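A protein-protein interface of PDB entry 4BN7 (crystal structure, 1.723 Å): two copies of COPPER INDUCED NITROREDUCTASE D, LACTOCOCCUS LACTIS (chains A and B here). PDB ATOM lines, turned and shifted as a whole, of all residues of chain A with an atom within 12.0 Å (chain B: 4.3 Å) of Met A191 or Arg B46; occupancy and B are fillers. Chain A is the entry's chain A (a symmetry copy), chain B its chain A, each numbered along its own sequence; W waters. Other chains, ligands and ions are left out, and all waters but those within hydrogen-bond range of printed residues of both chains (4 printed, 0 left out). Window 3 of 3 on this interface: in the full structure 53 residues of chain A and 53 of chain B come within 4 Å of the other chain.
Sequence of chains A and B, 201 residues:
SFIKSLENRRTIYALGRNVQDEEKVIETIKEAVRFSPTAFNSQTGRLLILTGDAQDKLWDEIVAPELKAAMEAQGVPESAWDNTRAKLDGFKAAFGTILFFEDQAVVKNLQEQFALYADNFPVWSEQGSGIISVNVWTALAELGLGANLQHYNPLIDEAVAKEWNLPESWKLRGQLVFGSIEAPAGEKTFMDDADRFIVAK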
ATOM      1  N   GLN A 127      -3.807 -32.700  17.055  1.00  0.00           N
ATOM      2  CA  GLN A 127      -3.103 -31.597  17.701  1.00  0.00           C
ATOM      3  C   GLN A 127      -1.896 -32.124  18.492  1.00  0.00           C
ATOM      4  O   GLN A 127      -0.794 -31.564  18.431  1.00  0.00           O
ATOM      5  CB  GLN A 127      -4.079 -30.802  18.586  1.00  0.00           C
ATOM      6  CG  GLN A 127      -5.143 -30.080  17.769  1.00  0.00           C
ATOM      7  CD  GLN A 127      -6.221 -29.429  18.602  1.00  0.00           C
ATOM      8  OE1 GLN A 127      -6.242 -29.554  19.829  1.00  0.00           O
ATOM      9  NE2 GLN A 127      -7.141 -28.735  17.934  1.00  0.00           N
ATOM     10  N   GLU A 187      15.651 -18.103   3.978  1.00  0.00           N
ATOM     11  CA  GLU A 187      14.923 -16.931   4.446  1.00  0.00           C
ATOM     12  C   GLU A 187      13.492 -17.310   4.793  1.00  0.00           C
ATOM     13  O   GLU A 187      12.921 -18.225   4.196  1.00  0.00           O
ATOM     14  CB  GLU A 187      14.912 -15.855   3.359  1.00  0.00           C
ATOM     15  CG  GLU A 187      16.273 -15.269   3.051  1.00  0.00           C
ATOM     16  CD  GLU A 187      16.290 -14.470   1.750  1.00  0.00           C
ATOM     17  OE1 GLU A 187      15.208 -14.215   1.170  1.00  0.00           O
ATOM     18  OE2 GLU A 187      17.397 -14.095   1.309  1.00  0.00           O
ATOM     19  N   LYS A 188      12.915 -16.613   5.766  1.00  0.00           N
ATOM     20  CA  LYS A 188      11.529 -16.838   6.143  1.00  0.00           C
ATOM     21  C   LYS A 188      10.860 -15.513   6.437  1.00  0.00           C
ATOM     22  O   LYS A 188      11.447 -14.635   7.057  1.00  0.00           O
ATOM     23  CB  LYS A 188      11.411 -17.738   7.376  1.00  0.00           C
ATOM     24  CG  LYS A 188       9.967 -18.018   7.756  1.00  0.00           C
ATOM     25  CD  LYS A 188       9.834 -19.090   8.819  1.00  0.00           C
ATOM     26  CE  LYS A 188      10.457 -18.661  10.120  1.00  0.00           C
ATOM     27  NZ  LYS A 188      10.174 -19.652  11.195  1.00  0.00           N
ATOM     28  N   THR A 189       9.626 -15.377   5.981  1.00  0.00           N
ATOM     29  CA  THR A 189       8.861 -14.165   6.235  1.00  0.00           C
ATOM     30  C   THR A 189       7.791 -14.419   7.290  1.00  0.00           C
ATOM     31  O   THR A 189       7.487 -15.568   7.636  1.00  0.00           O
ATOM     32  CB  THR A 189       8.189 -13.649   4.955  1.00  0.00           C
ATOM     33  OG1 THR A 189       7.277 -14.636   4.459  1.00  0.00           O
ATOM     34  CG2 THR A 189       9.237 -13.334   3.892  1.00  0.00           C
ATOM     35  N   PHE A 190       7.228 -13.331   7.796  1.00  0.00           N
ATOM     36  CA  PHE A 190       6.186 -13.384   8.809  1.00  0.00           C
ATOM     37  C   PHE A 190       5.063 -12.446   8.384  1.00  0.00           C
ATOM     38  O   PHE A 190       5.316 -11.381   7.821  1.00  0.00           O
ATOM     39  CB  PHE A 190       6.719 -12.940  10.174  1.00  0.00           C
ATOM     40  CG  PHE A 190       7.917 -13.716  10.647  1.00  0.00           C
ATOM     41  CD1 PHE A 190       9.196 -13.314  10.305  1.00  0.00           C
ATOM     42  CD2 PHE A 190       7.765 -14.837  11.447  1.00  0.00           C
ATOM     43  CE1 PHE A 190      10.297 -14.025  10.729  1.00  0.00           C
ATOM     44  CE2 PHE A 190       8.862 -15.542  11.887  1.00  0.00           C
ATOM     45  CZ  PHE A 190      10.134 -15.133  11.530  1.00  0.00           C
ATOM     46  N   MET A 191       3.829 -12.860   8.648  1.00  0.00           N
ATOM     47  CA  MET A 191       2.647 -12.025   8.469  1.00  0.00           C
ATOM     48  C   MET A 191       2.690 -10.766   9.320  1.00  0.00           C
ATOM     49  O   MET A 191       3.404 -10.700  10.320  1.00  0.00           O
ATOM     50  CB  MET A 191       1.421 -12.757   9.005  1.00  0.00           C
ATOM     51  CG  MET A 191       0.744 -13.763   8.142  1.00  0.00           C
ATOM     52  SD  MET A 191      -0.609 -14.380   9.169  1.00  0.00           S
ATOM     53  CE  MET A 191      -1.673 -12.943   9.256  1.00  0.00           C
ATOM     54  N   ASP A 192       1.845  -9.809   8.957  1.00  0.00           N
ATOM     55  CA  ASP A 192       1.570  -8.634   9.783  1.00  0.00           C
ATOM     56  C   ASP A 192       0.861  -9.053  11.078  1.00  0.00           C
ATOM     57  O   ASP A 192      -0.184  -9.714  11.041  1.00  0.00           O
ATOM     58  CB  ASP A 192       0.693  -7.667   8.973  1.00  0.00           C
ATOM     59  CG  ASP A 192       0.484  -6.322   9.647  1.00  0.00           C
ATOM     60  OD1 ASP A 192       0.703  -6.185  10.863  1.00  0.00           O
ATOM     61  OD2 ASP A 192       0.069  -5.385   8.941  1.00  0.00           O
ATOM     62  N   ASP A 193       1.437  -8.696  12.224  1.00  0.00           N
ATOM     63  CA  ASP A 193       0.777  -8.903  13.518  1.00  0.00           C
ATOM     64  C   ASP A 193      -0.710  -8.526  13.471  1.00  0.00           C
ATOM     65  O   ASP A 193      -1.563  -9.222  14.033  1.00  0.00           O
ATOM     66  CB  ASP A 193       1.439  -8.057  14.614  1.00  0.00           C
ATOM     67  CG  ASP A 193       2.780  -8.615  15.096  1.00  0.00           C
ATOM     68  OD1 ASP A 193       3.172  -9.742  14.723  1.00  0.00           O
ATOM     69  OD2 ASP A 193       3.452  -7.889  15.870  1.00  0.00           O
ATOM     70  N   ALA A 194      -1.014  -7.410  12.814  1.00  0.00           N
ATOM     71  CA  ALA A 194      -2.355  -6.839  12.858  1.00  0.00           C
ATOM     72  C   ALA A 194      -3.386  -7.765  12.235  1.00  0.00           C
ATOM     73  O   ALA A 194      -4.579  -7.654  12.517  1.00  0.00           O
ATOM     74  CB  ALA A 194      -2.382  -5.474  12.166  1.00  0.00           C
ATOM     75  N   ASP A 195      -2.928  -8.681  11.389  1.00  0.00           N
ATOM     76  CA  ASP A 195      -3.830  -9.594  10.699  1.00  0.00           C
ATOM     77  C   ASP A 195      -4.073 -10.911  11.450  1.00  0.00           C
ATOM     78  O   ASP A 195      -4.907 -11.711  11.031  1.00  0.00           O
ATOM     79  CB  ASP A 195      -3.307  -9.894   9.293  1.00  0.00           C
ATOM     80  CG  ASP A 195      -3.360  -8.688   8.377  1.00  0.00           C
ATOM     81  OD1 ASP A 195      -4.271  -7.841   8.528  1.00  0.00           O
ATOM     82  OD2 ASP A 195      -2.480  -8.593   7.503  1.00  0.00           O
ATOM     83  N   ARG A 196      -3.359 -11.153  12.547  1.00  0.00           N
ATOM     84  CA  ARG A 196      -3.575 -12.395  13.291  1.00  0.00           C
ATOM     85  C   ARG A 196      -3.662 -12.268  14.808  1.00  0.00           C
ATOM     86  O   ARG A 196      -3.956 -13.254  15.471  1.00  0.00           O
ATOM     87  CB  ARG A 196      -2.524 -13.451  12.936  1.00  0.00           C
ATOM     88  CG  ARG A 196      -1.090 -13.085  13.285  1.00  0.00           C
ATOM     89  CD  ARG A 196      -0.174 -14.305  13.125  1.00  0.00           C
ATOM     90  NE  ARG A 196       1.228 -13.931  12.978  1.00  0.00           N
ATOM     91  CZ  ARG A 196       2.214 -14.790  12.742  1.00  0.00           C
ATOM     92  NH1 ARG A 196       1.963 -16.084  12.651  1.00  0.00           N
ATOM     93  NH2 ARG A 196       3.457 -14.354  12.610  1.00  0.00           N
ATOM     94  N   PHE A 197      -3.405 -11.084  15.363  1.00  0.00           N
ATOM     95  CA  PHE A 197      -3.601 -10.877  16.795  1.00  0.00           C
ATOM     96  C   PHE A 197      -4.556  -9.729  17.066  1.00  0.00           C
ATOM     97  O   PHE A 197      -4.338  -8.614  16.594  1.00  0.00           O
ATOM     98  CB  PHE A 197      -2.284 -10.580  17.515  1.00  0.00           C
ATOM     99  CG  PHE A 197      -1.185 -11.552  17.222  1.00  0.00           C
ATOM    100  CD1 PHE A 197      -1.250 -12.865  17.659  1.00  0.00           C
ATOM    101  CD2 PHE A 197      -0.056 -11.139  16.533  1.00  0.00           C
ATOM    102  CE1 PHE A 197      -0.219 -13.745  17.395  1.00  0.00           C
ATOM    103  CE2 PHE A 197       0.969 -12.006  16.266  1.00  0.00           C
ATOM    104  CZ  PHE A 197       0.895 -13.317  16.691  1.00  0.00           C
ATOM    105  N   ILE A 198      -5.610 -10.013  17.829  1.00  0.00           N
ATOM    106  CA  ILE A 198      -6.511  -8.981  18.327  1.00  0.00           C
ATOM    107  C   ILE A 198      -6.454  -8.998  19.843  1.00  0.00           C
ATOM    108  O   ILE A 198      -6.621 -10.049  20.456  1.00  0.00           O
ATOM    109  CB  ILE A 198      -7.971  -9.246  17.916  1.00  0.00           C
ATOM    110  CG1 ILE A 198      -8.120  -9.201  16.398  1.00  0.00           C
ATOM    111  CG2 ILE A 198      -8.909  -8.227  18.578  1.00  0.00           C
ATOM    112  CD1 ILE A 198      -9.480  -9.663  15.919  1.00  0.00           C
ATOM    113  N   VAL A 199      -6.205  -7.840  20.443  1.00  0.00           N
ATOM    114  CA  VAL A 199      -6.192  -7.717  21.897  1.00  0.00           C
ATOM    115  C   VAL A 199      -7.364  -6.847  22.346  1.00  0.00           C
ATOM    116  O   VAL A 199      -7.584  -5.761  21.809  1.00  0.00           O
ATOM    117  CB  VAL A 199      -4.867  -7.094  22.393  1.00  0.00           C
ATOM    118  CG1 VAL A 199      -4.875  -6.941  23.904  1.00  0.00           C
ATOM    119  CG2 VAL A 199      -3.684  -7.927  21.945  1.00  0.00           C
ATOM    120  N   ALA A 200      -8.129  -7.330  23.323  1.00  0.00           N
ATOM    121  CA  ALA A 200      -9.264  -6.573  23.839  1.00  0.00           C
ATOM    122  C   ALA A 200      -9.225  -6.542  25.362  1.00  0.00           C
ATOM    123  O   ALA A 200      -8.848  -7.522  25.999  1.00  0.00           O
ATOM    124  CB  ALA A 200     -10.572  -7.181  23.352  1.00  0.00           C
ATOM    125  N   GLN B  43       0.954 -19.983   8.345  1.00  0.00           N
ATOM    126  CA  GLN B  43       0.613 -19.116   9.477  1.00  0.00           C
ATOM    127  C   GLN B  43      -0.893 -18.935   9.638  1.00  0.00           C
ATOM    128  O   GLN B  43      -1.399 -17.810   9.662  1.00  0.00           O
ATOM    129  CB  GLN B  43       1.287 -17.754   9.303  1.00  0.00           C
ATOM    130  CG  GLN B  43       2.801 -17.824   9.263  1.00  0.00           C
ATOM    131  CD  GLN B  43       3.418 -16.547   8.746  1.00  0.00           C
ATOM    132  OE1 GLN B  43       3.486 -15.544   9.457  1.00  0.00           O
ATOM    133  NE2 GLN B  43       3.859 -16.568   7.488  1.00  0.00           N
ATOM    134  N   THR B  44      -1.602 -20.052   9.772  1.00  0.00           N
ATOM    135  CA  THR B  44      -3.056 -20.046   9.775  1.00  0.00           C
ATOM    136  C   THR B  44      -3.662 -19.708  11.130  1.00  0.00           C
ATOM    137  O   THR B  44      -4.869 -19.497  11.230  1.00  0.00           O
ATOM    138  CB  THR B  44      -3.593 -21.411   9.343  1.00  0.00           C
ATOM    139  OG1 THR B  44      -2.847 -22.434  10.008  1.00  0.00           O
ATOM    140  CG2 THR B  44      -3.452 -21.577   7.849  1.00  0.00           C
ATOM    141  N   GLY B  45      -2.838 -19.648  12.169  1.00  0.00           N
ATOM    142  CA  GLY B  45      -3.344 -19.358  13.501  1.00  0.00           C
ATOM    143  C   GLY B  45      -3.770 -17.911  13.677  1.00  0.00           C
ATOM    144  O   GLY B  45      -3.120 -16.986  13.160  1.00  0.00           O
ATOM    145  N   ARG B  46      -4.866 -17.709  14.408  1.00  0.00           N
ATOM    146  CA  ARG B  46      -5.345 -16.372  14.749  1.00  0.00           C
ATOM    147  C   ARG B  46      -5.665 -16.342  16.235  1.00  0.00           C
ATOM    148  O   ARG B  46      -6.149 -17.333  16.778  1.00  0.00           O
ATOM    149  CB  ARG B  46      -6.605 -16.026  13.959  1.00  0.00           C
ATOM    150  CG  ARG B  46      -6.487 -16.186  12.459  1.00  0.00           C
ATOM    151  CD  ARG B  46      -5.739 -15.035  11.811  1.00  0.00           C
ATOM    152  NE  ARG B  46      -5.644 -15.219  10.367  1.00  0.00           N
ATOM    153  CZ  ARG B  46      -4.607 -15.766   9.739  1.00  0.00           C
ATOM    154  NH1 ARG B  46      -3.540 -16.179  10.409  1.00  0.00           N
ATOM    155  NH2 ARG B  46      -4.629 -15.881   8.425  1.00  0.00           N
ATOM    156  N   LEU B  47      -5.396 -15.220  16.896  1.00  0.00           N
ATOM    157  CA  LEU B  47      -5.632 -15.127  18.328  1.00  0.00           C
ATOM    158  C   LEU B  47      -6.494 -13.931  18.693  1.00  0.00           C
ATOM    159  O   LEU B  47      -6.318 -12.833  18.171  1.00  0.00           O
ATOM    160  CB  LEU B  47      -4.329 -15.015  19.099  1.00  0.00           C
ATOM    161  CG  LEU B  47      -3.520 -16.282  19.377  1.00  0.00           C
ATOM    162  CD1 LEU B  47      -2.989 -16.896  18.096  1.00  0.00           C
ATOM    163  CD2 LEU B  47      -2.385 -15.947  20.327  1.00  0.00           C
ATOM    164  N   LEU B  99      -8.066 -16.957  22.916  1.00  0.00           N
ATOM    165  CA  LEU B  99      -8.863 -17.799  22.039  1.00  0.00           C
ATOM    166  C   LEU B  99      -8.088 -18.056  20.756  1.00  0.00           C
ATOM    167  O   LEU B  99      -7.688 -17.124  20.073  1.00  0.00           O
ATOM    168  CB  LEU B  99     -10.218 -17.154  21.749  1.00  0.00           C
ATOM    169  CG  LEU B  99     -11.100 -17.071  23.004  1.00  0.00           C
ATOM    170  CD1 LEU B  99     -10.805 -15.794  23.778  1.00  0.00           C
ATOM    171  CD2 LEU B  99     -12.582 -17.186  22.698  1.00  0.00           C
ATOM    172  N   PHE B 100      -7.861 -19.336  20.470  1.00  0.00           N
ATOM    173  CA  PHE B 100      -7.085 -19.765  19.315  1.00  0.00           C
ATOM    174  C   PHE B 100      -8.014 -20.162  18.187  1.00  0.00           C
ATOM    175  O   PHE B 100      -8.924 -20.958  18.396  1.00  0.00           O
ATOM    176  CB  PHE B 100      -6.214 -20.957  19.702  1.00  0.00           C
ATOM    177  CG  PHE B 100      -5.038 -20.590  20.548  1.00  0.00           C
ATOM    178  CD1 PHE B 100      -3.840 -20.212  19.965  1.00  0.00           C
ATOM    179  CD2 PHE B 100      -5.126 -20.613  21.926  1.00  0.00           C
ATOM    180  CE1 PHE B 100      -2.754 -19.867  20.739  1.00  0.00           C
ATOM    181  CE2 PHE B 100      -4.040 -20.266  22.711  1.00  0.00           C
ATOM    182  CZ  PHE B 100      -2.851 -19.897  22.118  1.00  0.00           C
ATOM    183  N   PHE B 101      -7.790 -19.595  17.005  1.00  0.00           N
ATOM    184  CA  PHE B 101      -8.582 -19.923  15.821  1.00  0.00           C
ATOM    185  C   PHE B 101      -7.661 -20.383  14.692  1.00  0.00           C
ATOM    186  O   PHE B 101      -6.460 -20.101  14.699  1.00  0.00           O
ATOM    187  CB  PHE B 101      -9.350 -18.703  15.293  1.00  0.00           C
ATOM    188  CG  PHE B 101     -10.235 -18.016  16.306  1.00  0.00           C
ATOM    189  CD1 PHE B 101      -9.690 -17.197  17.283  1.00  0.00           C
ATOM    190  CD2 PHE B 101     -11.607 -18.154  16.246  1.00  0.00           C
ATOM    191  CE1 PHE B 101     -10.505 -16.545  18.197  1.00  0.00           C
ATOM    192  CE2 PHE B 101     -12.433 -17.505  17.153  1.00  0.00           C
ATOM    193  CZ  PHE B 101     -11.877 -16.700  18.136  1.00  0.00           C
ATOM    194  N   ASP B 103      -7.601 -19.996  10.468  1.00  0.00           N
ATOM    195  CA  ASP B 103      -8.225 -19.258   9.371  1.00  0.00           C
ATOM    196  C   ASP B 103      -8.566 -20.196   8.220  1.00  0.00           C
ATOM    197  O   ASP B 103      -7.685 -20.635   7.486  1.00  0.00           O
ATOM    198  CB  ASP B 103      -7.293 -18.148   8.884  1.00  0.00           C
ATOM    199  CG  ASP B 103      -7.984 -17.177   7.947  1.00  0.00           C
ATOM    200  OD1 ASP B 103      -8.992 -17.567   7.325  1.00  0.00           O
ATOM    201  OD2 ASP B 103      -7.519 -16.027   7.829  1.00  0.00           O
ATOM    202  N   VAL B 106      -7.607 -19.350   4.450  1.00  0.00           N
ATOM    203  CA  VAL B 106      -6.249 -19.681   4.035  1.00  0.00           C
ATOM    204  C   VAL B 106      -6.144 -21.173   3.728  1.00  0.00           C
ATOM    205  O   VAL B 106      -5.552 -21.569   2.728  1.00  0.00           O
ATOM    206  CB  VAL B 106      -5.232 -19.283   5.118  1.00  0.00           C
ATOM    207  CG1 VAL B 106      -3.843 -19.785   4.758  1.00  0.00           C
ATOM    208  CG2 VAL B 106      -5.236 -17.774   5.294  1.00  0.00           C
ATOM    209  N   TRP B 170     -12.551 -17.408  10.701  1.00  0.00           N
ATOM    210  CA  TRP B 170     -11.809 -17.828  11.893  1.00  0.00           C
ATOM    211  C   TRP B 170     -12.545 -18.952  12.633  1.00  0.00           C
ATOM    212  O   TRP B 170     -13.620 -18.735  13.199  1.00  0.00           O
ATOM    213  CB  TRP B 170     -11.595 -16.663  12.861  1.00  0.00           C
ATOM    214  CG  TRP B 170     -10.617 -15.607  12.421  1.00  0.00           C
ATOM    215  CD1 TRP B 170     -10.219 -15.315  11.146  1.00  0.00           C
ATOM    216  CD2 TRP B 170      -9.926 -14.689  13.274  1.00  0.00           C
ATOM    217  NE1 TRP B 170      -9.328 -14.266  11.160  1.00  0.00           N
ATOM    218  CE2 TRP B 170      -9.124 -13.873  12.456  1.00  0.00           C
ATOM    219  CE3 TRP B 170      -9.902 -14.485  14.657  1.00  0.00           C
ATOM    220  CZ2 TRP B 170      -8.315 -12.861  12.977  1.00  0.00           C
ATOM    221  CZ3 TRP B 170      -9.090 -13.491  15.171  1.00  0.00           C
ATOM    222  CH2 TRP B 170      -8.311 -12.690  14.333  1.00  0.00           C
HETATM  223  O   HOH W   1       4.859 -16.784  12.013  1.00  0.00           O
HETATM  224  O   HOH W   2      -0.408 -17.419  13.136  1.00  0.00           O
HETATM  225  O   HOH W   3       4.690 -14.334   5.526  1.00  0.00           O
HETATM  226  O   HOH W   4      -2.197 -16.808   6.952  1.00  0.00           O
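Of chain B, only Gln B43 and Arg B46 come within 4 Å of Met A191. Printed residues of chain A within 4 Å of Arg B46: Met A191, Asp A195 and Arg A196. Of chain A, only Thr A189, Phe A190, Met A191 and Arg A196 come within 4 Å of Gln B43. No residue of chain A comes within 4 Å of Thr B44. Leu B47 touches three residues of chain A. No residue of chain A comes within 4 Å of Phe B100. Phe B101 touches none of the printed residues of chain A. No residue of chain A comes within 4 Å of Asp B103. Of the printed residues of chain B, Ile A198 touches Leu B47 (2.9 Å) and Trp B170 (3.6 Å). Of the printed residues of chain B, Thr A189 touches Gln B43. The nearest printed residue of chain B that does not touch Met A191 is Gly B45 (5.4 Å). The nearest printed residue of chain B that does not touch Ile A198 is Arg B46 (6.5 Å).
Of the 15 printed residues of chain A, 7 touch a printed residue of chain B. Of the 11 printed residues of chain B, 5 touch a printed residue of chain A. Printed residues of chain B that touch a printed residue of chain A: Gln B43, Gly B45, Arg B46, Leu B47 and Trp B170. Hydrophobic or aromatic side chains of chain B that line the printed part of chain A: Trp B170. Among the printed residues, 12 pairs touch across the chains.
No position is printed for both chains. Of the 12 pairs that touch across the chains among the printed residues, none has its exchanged pair printed and touching as well.
O of Gln B43 is in hydrogen-bond range of NH1 of Arg B46, 2.8 Å away. The backbone carbonyl oxygen of Arg B46 is in hydrogen-bond range of the backbone NH of Phe B101, 2.8 Å away. The guanidinium group (NH2) of Arg B46 is in salt-bridge range of the side-chain carboxylate (OD2) of Asp B103 (3.0 Å).
Gln B43 touches Thr A189 (NE2 to O, 3.8 Å). Phe A190 touches Gln B43 (CA to OE1, 3.5 Å). CD of Arg B46 touches O of Asp A195, at 3.5 Å. CB of Arg A196 touches O of Gly B45, 3.6 Å away. CA of Arg B46 touches O of Arg A196 (3.5 Å). O of Leu B47 touches CA of Phe A197 (3.6 Å). Trp B170 touches Ile A198 (CH2 to CD1, 3.6 Å).
The guanidinium group (NH1) of Arg B46 is in hydrogen-bond range of the side-chain sulfur (SD) of Met A191 (3.7 Å). The guanidinium group of Arg A196 sits at hydrogen-bond distance from the side-chain amide oxygen of Gln B43 (3.4 Å). The backbone NH (N) of Ile A198 sits at hydrogen-bond distance from the backbone carbonyl oxygen (O) of Leu B47, 2.9 Å away. The backbone NH (N) of Leu B47 lies within hydrogen-bond range of the backbone carbonyl oxygen (O) of Arg A196 (2.8 Å). The side-chain amide oxygen of Gln B43 is in hydrogen-bond range of the backbone NH of Met A191 (2.8 Å).
Water W2 lies within hydrogen-bond range of O of Gly B45 (2.7 Å) and NH1 of Arg A196 (2.8 Å). Water W3 lies within hydrogen-bond range of the side-chain hydroxyl of Thr A189 (2.8 Å) and the side-chain amide nitrogen of Gln B43 (3.1 Å). Water W1 lies within hydrogen-bond range of the guanidinium group (NH2) of Arg A196 (2.9 Å) and the side-chain amide oxygen (OE1) of Gln B43 (3.2 Å). Water W4 lies within hydrogen-bond range of the guanidinium group (NH2) of Arg B46 (3.0 Å), the backbone carbonyl oxygen (O) of Gln B43 (3.0 Å) and the side-chain sulfur (SD) of Met A191 (3.7 Å).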
